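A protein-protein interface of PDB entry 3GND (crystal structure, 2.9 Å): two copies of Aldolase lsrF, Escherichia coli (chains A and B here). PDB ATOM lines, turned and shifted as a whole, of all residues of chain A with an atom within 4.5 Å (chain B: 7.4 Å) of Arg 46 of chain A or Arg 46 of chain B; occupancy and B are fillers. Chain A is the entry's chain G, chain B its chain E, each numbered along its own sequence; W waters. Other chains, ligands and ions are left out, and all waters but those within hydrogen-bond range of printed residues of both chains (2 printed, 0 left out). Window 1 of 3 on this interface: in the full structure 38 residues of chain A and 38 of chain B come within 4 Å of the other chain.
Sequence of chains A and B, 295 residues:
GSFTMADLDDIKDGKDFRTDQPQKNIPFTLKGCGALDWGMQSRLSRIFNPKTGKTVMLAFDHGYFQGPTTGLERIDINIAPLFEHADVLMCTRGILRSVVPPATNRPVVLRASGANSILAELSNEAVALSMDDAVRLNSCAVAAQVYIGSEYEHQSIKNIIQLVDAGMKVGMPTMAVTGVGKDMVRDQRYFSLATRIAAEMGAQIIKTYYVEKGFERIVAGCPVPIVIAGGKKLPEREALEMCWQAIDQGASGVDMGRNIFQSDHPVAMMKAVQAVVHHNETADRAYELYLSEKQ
O of Ser 45 of chain A lies within hydrogen-bond range of ND2 of Asn 105 of chain B (3.4 Å).
The guanidinium group of Arg 46 of chain A lies close to the guanidinium group of Arg 46 of chain B (3.5 Å).
The side-chain amide nitrogen (ND2) of Asn 138 of chain A sits at hydrogen-bond distance from the side-chain hydroxyl (OG) of Ser 42 of chain B, at 3.4 Å.
The side-chain amide oxygen (OD1) of Asn 138 of chain B is in hydrogen-bond range of the guanidinium group (NE) of Arg 43 of chain A (3.5 Å).
ND2 of Asn 138 of chain B is in hydrogen-bond range of OG of Ser 42 of chain A (3.2 Å).
O of Ser 45 of chain B is in hydrogen-bond range of ND2 of Asn 105 of chain A, 3.4 Å away.
NE of Arg 43 of chain B lies within hydrogen-bond range of OD1 of Asn 138 of chain A, at 3.3 Å.
O of Ser 139 of chain B is in hydrogen-bond range of NE of Arg 43 of chain B.
The guanidinium group (NH1) of Arg 46 of chain B sits at hydrogen-bond distance from the side-chain sulfur (SG) of Cys 140 of chain B, at 3.8 Å.
The side-chain sulfur of Cys 140 of chain A is in hydrogen-bond range of the guanidinium group of Arg 46 of chain A (3.7 Å).
OG of Ser 45 of chain B sits at hydrogen-bond distance from O of Gln 41 of chain B (2.9 Å).
Among the printed residues, pairs that only touch across the chains: Ser 45 of chain A with Pro 102 of chain B (3.8 Å), Arg 46 of chain A with Asn 105 of chain B (3.8 Å) and Asn 105 of chain A with Arg 46 of chain B (3.7 Å).
Arg 46 of chain A touches just these residues of chain B: Arg 46 (3.4 Å) and Asn 105 (3.8 Å).
Of the printed residues of chain B, Asn 105 of chain A touches Ser 45 and Arg 46.
Of the printed residues of chain B, Asn 138 of chain A touches Ser 42 (3.4 Å) and Arg 43 (3.3 Å).
Cys 140 of chain A touches none of the printed residues of chain B.
Printed residues of chain A within 4 Å of Arg 43 of chain B: Asn 138 (3.3 Å).
Of chain A, only Arg 46 and Asn 105 come within 4 Å of Arg 46 of chain B.
Lys 54 of chain B touches none of the printed residues of chain A.
Printed residues of chain A within 4 Å of Asn 105 of chain B: Ser 45 (3.4 Å) and Arg 46 (3.8 Å).
Printed residues of chain A within 4 Å of Asn 138 of chain B: Ser 42 (3.2 Å) and Arg 43 (3.5 Å).
The nearest residue of chain B that does not touch Arg 46 of chain A is Asn 138 of chain B (4.1 Å).
The nearest printed residue of chain A that does not touch Asn 138 of chain B is Asn 138 of chain A (4.1 Å).
Printed residues of chain A that touch a printed residue of chain B: Ser 42, Arg 43, Ser 45, Arg 46, Asn 105 and Asn 138.
Of the 23 printed residues of chain B, 7 touch a printed residue of chain A.
Among the printed residues, no Asp or Glu carboxylate lies within 4 Å of a Lys or Arg side-chain nitrogen of the other chain.
Ser 42 of chain A touches Asn 138 of chain B, and with the chains exchanged Asn 138 of chain A touches Ser 42 of chain B.
Ser 45 of chain A touches Asn 105 of chain B, and with the chains exchanged Asn 105 of chain A touches Ser 45 of chain B.
Arg 46 of chain B touches its own counterpart, Arg 46 of chain A.
Arg 46 of chain A touches Asn 105 of chain B, and with the chains exchanged Asn 105 of chain A touches Arg 46 of chain B.
Of the 10 pairs that touch across the chains among the printed residues, 9 have their exchanged pair printed and touching as well.
Water W2 lies within hydrogen-bond range of OD1 of Asn 105 of chain B, O of Ser 42 of chain A and N of Arg 46 of chain A.
Water W1 bridges OD1 of Asn 105 of chain A (2.7 Å) and O of Ser 42 of chain B (3.0 Å).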
ATOM      1  N   SER A  42     -29.540 -18.362  16.855  1.00  0.00           N
ATOM      2  CA  SER A  42     -29.697 -19.795  16.904  1.00  0.00           C
ATOM      3  C   SER A  42     -28.356 -20.455  17.209  1.00  0.00           C
ATOM      4  O   SER A  42     -28.260 -21.303  18.090  1.00  0.00           O
ATOM      5  CB  SER A  42     -30.230 -20.253  15.563  1.00  0.00           C
ATOM      6  OG  SER A  42     -30.200 -21.648  15.484  1.00  0.00           O
ATOM      7  N   ARG A  43     -27.311 -20.058  16.500  1.00  0.00           N
ATOM      8  CA  ARG A  43     -26.011 -20.636  16.768  1.00  0.00           C
ATOM      9  C   ARG A  43     -25.620 -20.307  18.201  1.00  0.00           C
ATOM     10  O   ARG A  43     -25.108 -21.173  18.906  1.00  0.00           O
ATOM     11  CB  ARG A  43     -24.938 -20.117  15.798  1.00  0.00           C
ATOM     12  CG  ARG A  43     -25.174 -20.478  14.326  1.00  0.00           C
ATOM     13  CD  ARG A  43     -24.011 -20.061  13.421  1.00  0.00           C
ATOM     14  NE  ARG A  43     -24.104 -20.814  12.168  1.00  0.00           N
ATOM     15  CZ  ARG A  43     -24.674 -20.368  11.062  1.00  0.00           C
ATOM     16  NH1 ARG A  43     -25.187 -19.147  11.001  1.00  0.00           N
ATOM     17  NH2 ARG A  43     -24.705 -21.130  10.004  1.00  0.00           N
ATOM     18  N   LEU A  44     -25.861 -19.072  18.643  1.00  0.00           N
ATOM     19  CA  LEU A  44     -25.476 -18.690  19.994  1.00  0.00           C
ATOM     20  C   LEU A  44     -26.225 -19.509  21.022  1.00  0.00           C
ATOM     21  O   LEU A  44     -25.708 -19.784  22.095  1.00  0.00           O
ATOM     22  CB  LEU A  44     -25.729 -17.206  20.243  1.00  0.00           C
ATOM     23  CG  LEU A  44     -24.792 -16.251  19.512  1.00  0.00           C
ATOM     24  CD1 LEU A  44     -25.303 -14.867  19.661  1.00  0.00           C
ATOM     25  CD2 LEU A  44     -23.371 -16.372  20.062  1.00  0.00           C
ATOM     26  N   SER A  45     -27.448 -19.902  20.698  1.00  0.00           N
ATOM     27  CA  SER A  45     -28.258 -20.676  21.645  1.00  0.00           C
ATOM     28  C   SER A  45     -27.799 -22.118  21.690  1.00  0.00           C
ATOM     29  O   SER A  45     -28.123 -22.844  22.626  1.00  0.00           O
ATOM     30  CB  SER A  45     -29.748 -20.648  21.297  1.00  0.00           C
ATOM     31  OG  SER A  45     -30.261 -19.335  21.310  1.00  0.00           O
ATOM     32  N   ARG A  46     -27.074 -22.561  20.669  1.00  0.00           N
ATOM     33  CA  ARG A  46     -26.449 -23.889  20.761  1.00  0.00           C
ATOM     34  C   ARG A  46     -25.307 -23.877  21.790  1.00  0.00           C
ATOM     35  O   ARG A  46     -25.044 -24.886  22.425  1.00  0.00           O
ATOM     36  CB  ARG A  46     -25.940 -24.363  19.403  1.00  0.00           C
ATOM     37  CG  ARG A  46     -27.052 -24.584  18.411  1.00  0.00           C
ATOM     38  CD  ARG A  46     -26.601 -25.417  17.229  1.00  0.00           C
ATOM     39  NE  ARG A  46     -26.191 -26.754  17.624  1.00  0.00           N
ATOM     40  CZ  ARG A  46     -25.411 -27.544  16.895  1.00  0.00           C
ATOM     41  NH1 ARG A  46     -24.921 -27.155  15.728  1.00  0.00           N
ATOM     42  NH2 ARG A  46     -25.115 -28.738  17.345  1.00  0.00           N
ATOM     43  N   ILE A  47     -24.651 -22.719  21.941  1.00  0.00           N
ATOM     44  CA  ILE A  47     -23.480 -22.546  22.792  1.00  0.00           C
ATOM     45  C   ILE A  47     -23.951 -22.207  24.199  1.00  0.00           C
ATOM     46  O   ILE A  47     -23.544 -22.875  25.148  1.00  0.00           O
ATOM     47  CB  ILE A  47     -22.513 -21.428  22.246  1.00  0.00           C
ATOM     48  CG1 ILE A  47     -21.848 -21.872  20.951  1.00  0.00           C
ATOM     49  CG2 ILE A  47     -21.421 -21.064  23.235  1.00  0.00           C
ATOM     50  CD1 ILE A  47     -21.134 -20.749  20.238  1.00  0.00           C
ATOM     51  N   PHE A  48     -24.799 -21.185  24.343  1.00  0.00           N
ATOM     52  CA  PHE A  48     -25.252 -20.772  25.654  1.00  0.00           C
ATOM     53  C   PHE A  48     -26.646 -21.293  25.933  1.00  0.00           C
ATOM     54  O   PHE A  48     -27.619 -20.863  25.352  1.00  0.00           O
ATOM     55  CB  PHE A  48     -25.232 -19.259  25.763  1.00  0.00           C
ATOM     56  CG  PHE A  48     -23.865 -18.667  25.620  1.00  0.00           C
ATOM     57  CD1 PHE A  48     -22.993 -18.598  26.715  1.00  0.00           C
ATOM     58  CD2 PHE A  48     -23.450 -18.181  24.399  1.00  0.00           C
ATOM     59  CE1 PHE A  48     -21.725 -18.062  26.578  1.00  0.00           C
ATOM     60  CE2 PHE A  48     -22.180 -17.644  24.246  1.00  0.00           C
ATOM     61  CZ  PHE A  48     -21.307 -17.580  25.336  1.00  0.00           C
ATOM     62  N   ASN A 105     -22.557 -35.296  17.729  1.00  0.00           N
ATOM     63  CA  ASN A 105     -23.705 -34.412  17.854  1.00  0.00           C
ATOM     64  C   ASN A 105     -23.556 -33.354  18.922  1.00  0.00           C
ATOM     65  O   ASN A 105     -24.442 -33.135  19.724  1.00  0.00           O
ATOM     66  CB  ASN A 105     -24.962 -35.229  18.102  1.00  0.00           C
ATOM     67  CG  ASN A 105     -26.228 -34.468  17.757  1.00  0.00           C
ATOM     68  OD1 ASN A 105     -26.213 -33.457  17.068  1.00  0.00           O
ATOM     69  ND2 ASN A 105     -27.336 -34.974  18.230  1.00  0.00           N
ATOM     70  N   ARG A 106     -22.440 -32.661  18.902  1.00  0.00           N
ATOM     71  CA  ARG A 106     -22.166 -31.621  19.877  1.00  0.00           C
ATOM     72  C   ARG A 106     -21.744 -30.346  19.134  1.00  0.00           C
ATOM     73  O   ARG A 106     -21.011 -30.410  18.139  1.00  0.00           O
ATOM     74  CB  ARG A 106     -21.039 -32.145  20.766  1.00  0.00           C
ATOM     75  CG  ARG A 106     -21.055 -31.677  22.185  1.00  0.00           C
ATOM     76  CD  ARG A 106     -22.352 -32.012  22.920  1.00  0.00           C
ATOM     77  NE  ARG A 106     -22.582 -33.436  23.002  1.00  0.00           N
ATOM     78  CZ  ARG A 106     -23.487 -33.976  23.800  1.00  0.00           C
ATOM     79  NH1 ARG A 106     -24.209 -33.198  24.573  1.00  0.00           N
ATOM     80  NH2 ARG A 106     -23.659 -35.281  23.848  1.00  0.00           N
ATOM     81  N   PRO A 107     -22.208 -29.187  19.577  1.00  0.00           N
ATOM     82  CA  PRO A 107     -21.848 -27.925  18.886  1.00  0.00           C
ATOM     83  C   PRO A 107     -20.348 -27.616  18.949  1.00  0.00           C
ATOM     84  O   PRO A 107     -19.730 -27.885  19.954  1.00  0.00           O
ATOM     85  CB  PRO A 107     -22.622 -26.848  19.643  1.00  0.00           C
ATOM     86  CG  PRO A 107     -23.435 -27.548  20.676  1.00  0.00           C
ATOM     87  CD  PRO A 107     -23.082 -29.001  20.732  1.00  0.00           C
ATOM     88  N   ASN A 138     -20.253 -26.632   9.538  1.00  0.00           N
ATOM     89  CA  ASN A 138     -21.409 -26.444  10.431  1.00  0.00           C
ATOM     90  C   ASN A 138     -21.036 -25.852  11.796  1.00  0.00           C
ATOM     91  O   ASN A 138     -21.607 -26.273  12.804  1.00  0.00           O
ATOM     92  CB  ASN A 138     -22.129 -27.773  10.657  1.00  0.00           C
ATOM     93  CG  ASN A 138     -23.500 -27.594  11.254  1.00  0.00           C
ATOM     94  OD1 ASN A 138     -24.125 -26.548  11.059  1.00  0.00           O
ATOM     95  ND2 ASN A 138     -23.999 -28.623  11.985  1.00  0.00           N
ATOM     96  N   CYS A 140     -20.683 -23.358  15.093  1.00  0.00           N
ATOM     97  CA  CYS A 140     -21.482 -22.416  15.849  1.00  0.00           C
ATOM     98  C   CYS A 140     -20.758 -21.110  16.052  1.00  0.00           C
ATOM     99  O   CYS A 140     -21.406 -20.094  16.284  1.00  0.00           O
ATOM    100  CB  CYS A 140     -21.785 -22.973  17.208  1.00  0.00           C
ATOM    101  SG  CYS A 140     -22.811 -24.436  17.082  1.00  0.00           S
ATOM    102  N   MET B  40     -21.439 -31.964   6.763  1.00  0.00           N
ATOM    103  CA  MET B  40     -22.717 -32.438   6.284  1.00  0.00           C
ATOM    104  C   MET B  40     -23.207 -33.605   7.153  1.00  0.00           C
ATOM    105  O   MET B  40     -24.405 -33.763   7.423  1.00  0.00           O
ATOM    106  CB  MET B  40     -22.643 -32.835   4.801  1.00  0.00           C
ATOM    107  CG  MET B  40     -24.000 -33.227   4.228  1.00  0.00           C
ATOM    108  SD  MET B  40     -24.047 -33.408   2.442  1.00  0.00           S
ATOM    109  CE  MET B  40     -24.289 -31.711   1.946  1.00  0.00           C
ATOM    110  N   GLN B  41     -22.265 -34.420   7.598  1.00  0.00           N
ATOM    111  CA  GLN B  41     -22.642 -35.521   8.453  1.00  0.00           C
ATOM    112  C   GLN B  41     -23.068 -34.958   9.783  1.00  0.00           C
ATOM    113  O   GLN B  41     -23.924 -35.492  10.445  1.00  0.00           O
ATOM    114  CB  GLN B  41     -21.493 -36.513   8.605  1.00  0.00           C
ATOM    115  CG  GLN B  41     -21.187 -37.281   7.325  1.00  0.00           C
ATOM    116  CD  GLN B  41     -20.069 -38.252   7.513  1.00  0.00           C
ATOM    117  OE1 GLN B  41     -19.090 -37.981   8.211  1.00  0.00           O
ATOM    118  NE2 GLN B  41     -20.201 -39.398   6.890  1.00  0.00           N
ATOM    119  N   SER B  42     -22.474 -33.856  10.173  1.00  0.00           N
ATOM    120  CA  SER B  42     -22.852 -33.206  11.412  1.00  0.00           C
ATOM    121  C   SER B  42     -24.307 -32.740  11.379  1.00  0.00           C
ATOM    122  O   SER B  42     -25.075 -32.999  12.321  1.00  0.00           O
ATOM    123  CB  SER B  42     -21.925 -32.013  11.685  1.00  0.00           C
ATOM    124  OG  SER B  42     -22.246 -31.347  12.901  1.00  0.00           O
ATOM    125  N   ARG B  43     -24.677 -32.031  10.315  1.00  0.00           N
ATOM    126  CA  ARG B  43     -26.038 -31.570  10.160  1.00  0.00           C
ATOM    127  C   ARG B  43     -26.989 -32.737  10.156  1.00  0.00           C
ATOM    128  O   ARG B  43     -28.037 -32.673  10.792  1.00  0.00           O
ATOM    129  CB  ARG B  43     -26.214 -30.728   8.897  1.00  0.00           C
ATOM    130  CG  ARG B  43     -25.470 -29.399   8.935  1.00  0.00           C
ATOM    131  CD  ARG B  43     -25.783 -28.528   7.748  1.00  0.00           C
ATOM    132  NE  ARG B  43     -25.289 -27.181   7.986  1.00  0.00           N
ATOM    133  CZ  ARG B  43     -24.150 -26.688   7.494  1.00  0.00           C
ATOM    134  NH1 ARG B  43     -23.369 -27.436   6.719  1.00  0.00           N
ATOM    135  NH2 ARG B  43     -23.783 -25.432   7.762  1.00  0.00           N
ATOM    136  N   LEU B  44     -26.640 -33.807   9.456  1.00  0.00           N
ATOM    137  CA  LEU B  44     -27.524 -34.979   9.418  1.00  0.00           C
ATOM    138  C   LEU B  44     -27.699 -35.607  10.802  1.00  0.00           C
ATOM    139  O   LEU B  44     -28.776 -36.092  11.136  1.00  0.00           O
ATOM    140  CB  LEU B  44     -27.019 -36.027   8.451  1.00  0.00           C
ATOM    141  CG  LEU B  44     -27.152 -35.637   6.995  1.00  0.00           C
ATOM    142  CD1 LEU B  44     -26.349 -36.613   6.159  1.00  0.00           C
ATOM    143  CD2 LEU B  44     -28.589 -35.632   6.566  1.00  0.00           C
ATOM    144  N   SER B  45     -26.635 -35.576  11.603  1.00  0.00           N
ATOM    145  CA  SER B  45     -26.659 -36.140  12.943  1.00  0.00           C
ATOM    146  C   SER B  45     -27.458 -35.298  13.903  1.00  0.00           C
ATOM    147  O   SER B  45     -27.781 -35.753  14.994  1.00  0.00           O
ATOM    148  CB  SER B  45     -25.250 -36.279  13.505  1.00  0.00           C
ATOM    149  OG  SER B  45     -24.506 -37.198  12.748  1.00  0.00           O
ATOM    150  N   ARG B  46     -27.730 -34.059  13.528  1.00  0.00           N
ATOM    151  CA  ARG B  46     -28.664 -33.226  14.287  1.00  0.00           C
ATOM    152  C   ARG B  46     -30.097 -33.663  14.035  1.00  0.00           C
ATOM    153  O   ARG B  46     -30.928 -33.527  14.901  1.00  0.00           O
ATOM    154  CB  ARG B  46     -28.508 -31.739  13.923  1.00  0.00           C
ATOM    155  CG  ARG B  46     -27.193 -31.135  14.406  1.00  0.00           C
ATOM    156  CD  ARG B  46     -27.296 -29.650  14.501  1.00  0.00           C
ATOM    157  NE  ARG B  46     -28.179 -29.164  15.560  1.00  0.00           N
ATOM    158  CZ  ARG B  46     -28.648 -27.911  15.611  1.00  0.00           C
ATOM    159  NH1 ARG B  46     -28.330 -27.028  14.677  1.00  0.00           N
ATOM    160  NH2 ARG B  46     -29.439 -27.530  16.589  1.00  0.00           N
ATOM    161  N   ILE B  47     -30.348 -34.213  12.852  1.00  0.00           N
ATOM    162  CA  ILE B  47     -31.662 -34.636  12.449  1.00  0.00           C
ATOM    163  C   ILE B  47     -31.900 -36.112  12.826  1.00  0.00           C
ATOM    164  O   ILE B  47     -32.951 -36.467  13.390  1.00  0.00           O
ATOM    165  CB  ILE B  47     -31.856 -34.456  10.926  1.00  0.00           C
ATOM    166  CG1 ILE B  47     -31.765 -32.974  10.502  1.00  0.00           C
ATOM    167  CG2 ILE B  47     -33.162 -35.126  10.451  1.00  0.00           C
ATOM    168  CD1 ILE B  47     -31.561 -32.770   8.968  1.00  0.00           C
ATOM    169  N   PHE B  48     -30.952 -36.991  12.499  1.00  0.00           N
ATOM    170  CA  PHE B  48     -31.108 -38.416  12.818  1.00  0.00           C
ATOM    171  C   PHE B  48     -30.240 -38.812  14.004  1.00  0.00           C
ATOM    172  O   PHE B  48     -29.010 -38.895  13.906  1.00  0.00           O
ATOM    173  CB  PHE B  48     -30.773 -39.290  11.623  1.00  0.00           C
ATOM    174  CG  PHE B  48     -31.619 -39.013  10.421  1.00  0.00           C
ATOM    175  CD1 PHE B  48     -32.842 -39.658  10.254  1.00  0.00           C
ATOM    176  CD2 PHE B  48     -31.203 -38.105   9.451  1.00  0.00           C
ATOM    177  CE1 PHE B  48     -33.643 -39.422   9.135  1.00  0.00           C
ATOM    178  CE2 PHE B  48     -31.992 -37.844   8.336  1.00  0.00           C
ATOM    179  CZ  PHE B  48     -33.223 -38.502   8.172  1.00  0.00           C
ATOM    180  N   ASN B  49     -30.911 -39.062  15.123  1.00  0.00           N
ATOM    181  CA  ASN B  49     -30.280 -39.518  16.338  1.00  0.00           C
ATOM    182  C   ASN B  49     -29.256 -40.590  16.055  1.00  0.00           C
ATOM    183  O   ASN B  49     -29.619 -41.681  15.626  1.00  0.00           O
ATOM    184  CB  ASN B  49     -31.339 -40.070  17.284  1.00  0.00           C
ATOM    185  CG  ASN B  49     -30.767 -40.444  18.633  1.00  0.00           C
ATOM    186  OD1 ASN B  49     -29.639 -40.913  18.736  1.00  0.00           O
ATOM    187  ND2 ASN B  49     -31.543 -40.233  19.674  1.00  0.00           N
ATOM    188  N   PRO B  50     -27.967 -40.287  16.318  1.00  0.00           N
ATOM    189  CA  PRO B  50     -26.846 -41.201  16.059  1.00  0.00           C
ATOM    190  C   PRO B  50     -27.048 -42.576  16.698  1.00  0.00           C
ATOM    191  O   PRO B  50     -26.665 -43.575  16.110  1.00  0.00           O
ATOM    192  CB  PRO B  50     -25.658 -40.496  16.698  1.00  0.00           C
ATOM    193  CG  PRO B  50     -26.046 -39.066  16.734  1.00  0.00           C
ATOM    194  CD  PRO B  50     -27.525 -39.037  16.963  1.00  0.00           C
ATOM    195  N   LYS B  54     -32.785 -42.551  13.743  1.00  0.00           N
ATOM    196  CA  LYS B  54     -34.131 -42.182  13.324  1.00  0.00           C
ATOM    197  C   LYS B  54     -34.465 -40.792  13.824  1.00  0.00           C
ATOM    198  O   LYS B  54     -33.708 -40.191  14.576  1.00  0.00           O
ATOM    199  CB  LYS B  54     -35.165 -43.173  13.874  1.00  0.00           C
ATOM    200  CG  LYS B  54     -34.991 -44.602  13.410  1.00  0.00           C
ATOM    201  CD  LYS B  54     -35.860 -45.508  14.229  1.00  0.00           C
ATOM    202  CE  LYS B  54     -35.460 -46.955  14.052  1.00  0.00           C
ATOM    203  NZ  LYS B  54     -35.282 -47.206  12.610  1.00  0.00           N
ATOM    204  N   THR B  55     -35.620 -40.289  13.420  1.00  0.00           N
ATOM    205  CA  THR B  55     -35.998 -38.922  13.752  1.00  0.00           C
ATOM    206  C   THR B  55     -37.507 -38.737  13.837  1.00  0.00           C
ATOM    207  O   THR B  55     -38.255 -39.290  13.034  1.00  0.00           O
ATOM    208  CB  THR B  55     -35.456 -37.907  12.694  1.00  0.00           C
ATOM    209  OG1 THR B  55     -35.636 -36.561  13.152  1.00  0.00           O
ATOM    210  CG2 THR B  55     -36.172 -38.104  11.370  1.00  0.00           C
ATOM    211  N   ASP B  87     -37.799 -33.684  17.741  1.00  0.00           N
ATOM    212  CA  ASP B  87     -36.382 -33.831  17.427  1.00  0.00           C
ATOM    213  C   ASP B  87     -35.927 -32.719  16.475  1.00  0.00           C
ATOM    214  O   ASP B  87     -34.843 -32.130  16.635  1.00  0.00           O
ATOM    215  CB  ASP B  87     -36.109 -35.175  16.749  1.00  0.00           C
ATOM    216  CG  ASP B  87     -36.332 -36.365  17.668  1.00  0.00           C
ATOM    217  OD1 ASP B  87     -36.544 -36.152  18.869  1.00  0.00           O
ATOM    218  OD2 ASP B  87     -36.302 -37.522  17.187  1.00  0.00           O
ATOM    219  N   VAL B  88     -36.750 -32.447  15.471  1.00  0.00           N
ATOM    220  CA  VAL B  88     -36.461 -31.369  14.527  1.00  0.00           C
ATOM    221  C   VAL B  88     -37.752 -30.667  14.054  1.00  0.00           C
ATOM    222  O   VAL B  88     -38.815 -31.297  13.974  1.00  0.00           O
ATOM    223  CB  VAL B  88     -35.633 -31.863  13.320  1.00  0.00           C
ATOM    224  CG1 VAL B  88     -36.141 -33.173  12.847  1.00  0.00           C
ATOM    225  CG2 VAL B  88     -35.733 -30.873  12.192  1.00  0.00           C
ATOM    226  N   PRO B 102     -35.681 -18.399  18.672  1.00  0.00           N
ATOM    227  CA  PRO B 102     -34.368 -18.998  18.441  1.00  0.00           C
ATOM    228  C   PRO B 102     -33.941 -19.840  19.648  1.00  0.00           C
ATOM    229  O   PRO B 102     -33.250 -20.848  19.486  1.00  0.00           O
ATOM    230  CB  PRO B 102     -33.450 -17.773  18.274  1.00  0.00           C
ATOM    231  CG  PRO B 102     -34.322 -16.693  17.908  1.00  0.00           C
ATOM    232  CD  PRO B 102     -35.624 -16.932  18.593  1.00  0.00           C
ATOM    233  N   ASN B 105     -33.776 -23.759  20.578  1.00  0.00           N
ATOM    234  CA  ASN B 105     -32.643 -24.672  20.489  1.00  0.00           C
ATOM    235  C   ASN B 105     -33.003 -26.036  19.914  1.00  0.00           C
ATOM    236  O   ASN B 105     -32.637 -27.079  20.473  1.00  0.00           O
ATOM    237  CB  ASN B 105     -31.981 -24.842  21.858  1.00  0.00           C
ATOM    238  CG  ASN B 105     -30.544 -25.293  21.755  1.00  0.00           C
ATOM    239  OD1 ASN B 105     -29.950 -25.238  20.707  1.00  0.00           O
ATOM    240  ND2 ASN B 105     -29.985 -25.724  22.854  1.00  0.00           N
ATOM    241  N   ARG B 106     -33.702 -26.039  18.787  1.00  0.00           N
ATOM    242  CA  ARG B 106     -34.095 -27.287  18.155  1.00  0.00           C
ATOM    243  C   ARG B 106     -33.706 -27.220  16.677  1.00  0.00           C
ATOM    244  O   ARG B 106     -33.880 -26.183  16.070  1.00  0.00           O
ATOM    245  CB  ARG B 106     -35.593 -27.392  18.306  1.00  0.00           C
ATOM    246  CG  ARG B 106     -36.136 -28.769  18.391  1.00  0.00           C
ATOM    247  CD  ARG B 106     -35.536 -29.556  19.506  1.00  0.00           C
ATOM    248  NE  ARG B 106     -35.815 -28.980  20.798  1.00  0.00           N
ATOM    249  CZ  ARG B 106     -35.680 -29.641  21.935  1.00  0.00           C
ATOM    250  NH1 ARG B 106     -35.288 -30.896  21.907  1.00  0.00           N
ATOM    251  NH2 ARG B 106     -35.943 -29.063  23.092  1.00  0.00           N
ATOM    252  N   PRO B 107     -33.147 -28.296  16.092  1.00  0.00           N
ATOM    253  CA  PRO B 107     -32.691 -28.259  14.687  1.00  0.00           C
ATOM    254  C   PRO B 107     -33.848 -28.008  13.742  1.00  0.00           C
ATOM    255  O   PRO B 107     -34.914 -28.544  13.957  1.00  0.00           O
ATOM    256  CB  PRO B 107     -32.128 -29.669  14.440  1.00  0.00           C
ATOM    257  CG  PRO B 107     -32.060 -30.331  15.716  1.00  0.00           C
ATOM    258  CD  PRO B 107     -32.890 -29.593  16.729  1.00  0.00           C
ATOM    259  N   VAL B 108     -33.654 -27.203  12.699  1.00  0.00           N
ATOM    260  CA  VAL B 108     -34.738 -26.951  11.714  1.00  0.00           C
ATOM    261  C   VAL B 108     -34.445 -27.464  10.297  1.00  0.00           C
ATOM    262  O   VAL B 108     -33.291 -27.502   9.851  1.00  0.00           O
ATOM    263  CB  VAL B 108     -35.048 -25.466  11.604  1.00  0.00           C
ATOM    264  CG1 VAL B 108     -35.495 -24.938  12.948  1.00  0.00           C
ATOM    265  CG2 VAL B 108     -33.813 -24.729  11.146  1.00  0.00           C
ATOM    266  N   ASN B 138     -28.896 -20.973   9.800  1.00  0.00           N
ATOM    267  CA  ASN B 138     -28.340 -22.112  10.508  1.00  0.00           C
ATOM    268  C   ASN B 138     -29.179 -23.388  10.316  1.00  0.00           C
ATOM    269  O   ASN B 138     -29.326 -24.178  11.248  1.00  0.00           O
ATOM    270  CB  ASN B 138     -28.243 -21.800  12.016  1.00  0.00           C
ATOM    271  CG  ASN B 138     -27.390 -22.809  12.778  1.00  0.00           C
ATOM    272  OD1 ASN B 138     -26.462 -23.359  12.232  1.00  0.00           O
ATOM    273  ND2 ASN B 138     -27.701 -23.035  14.038  1.00  0.00           N
ATOM    274  N   SER B 139     -29.727 -23.600   9.128  1.00  0.00           N
ATOM    275  CA  SER B 139     -30.483 -24.809   8.856  1.00  0.00           C
ATOM    276  C   SER B 139     -29.665 -26.073   8.939  1.00  0.00           C
ATOM    277  O   SER B 139     -28.476 -26.047   8.692  1.00  0.00           O
ATOM    278  CB  SER B 139     -31.015 -24.779   7.446  1.00  0.00           C
ATOM    279  OG  SER B 139     -31.911 -23.712   7.283  1.00  0.00           O
ATOM    280  N   CYS B 140     -30.333 -27.188   9.218  1.00  0.00           N
ATOM    281  CA  CYS B 140     -29.748 -28.502   9.093  1.00  0.00           C
ATOM    282  C   CYS B 140     -30.023 -29.103   7.719  1.00  0.00           C
ATOM    283  O   CYS B 140     -29.376 -30.074   7.336  1.00  0.00           O
ATOM    284  CB  CYS B 140     -30.318 -29.419  10.144  1.00  0.00           C
ATOM    285  SG  CYS B 140     -29.847 -28.921  11.792  1.00  0.00           S
HETATM  286  O   HOH W   1     -24.615 -32.435  15.196  1.00  0.00           O
HETATM  287  O   HOH W   2     -29.756 -23.409  18.886  1.00  0.00           O
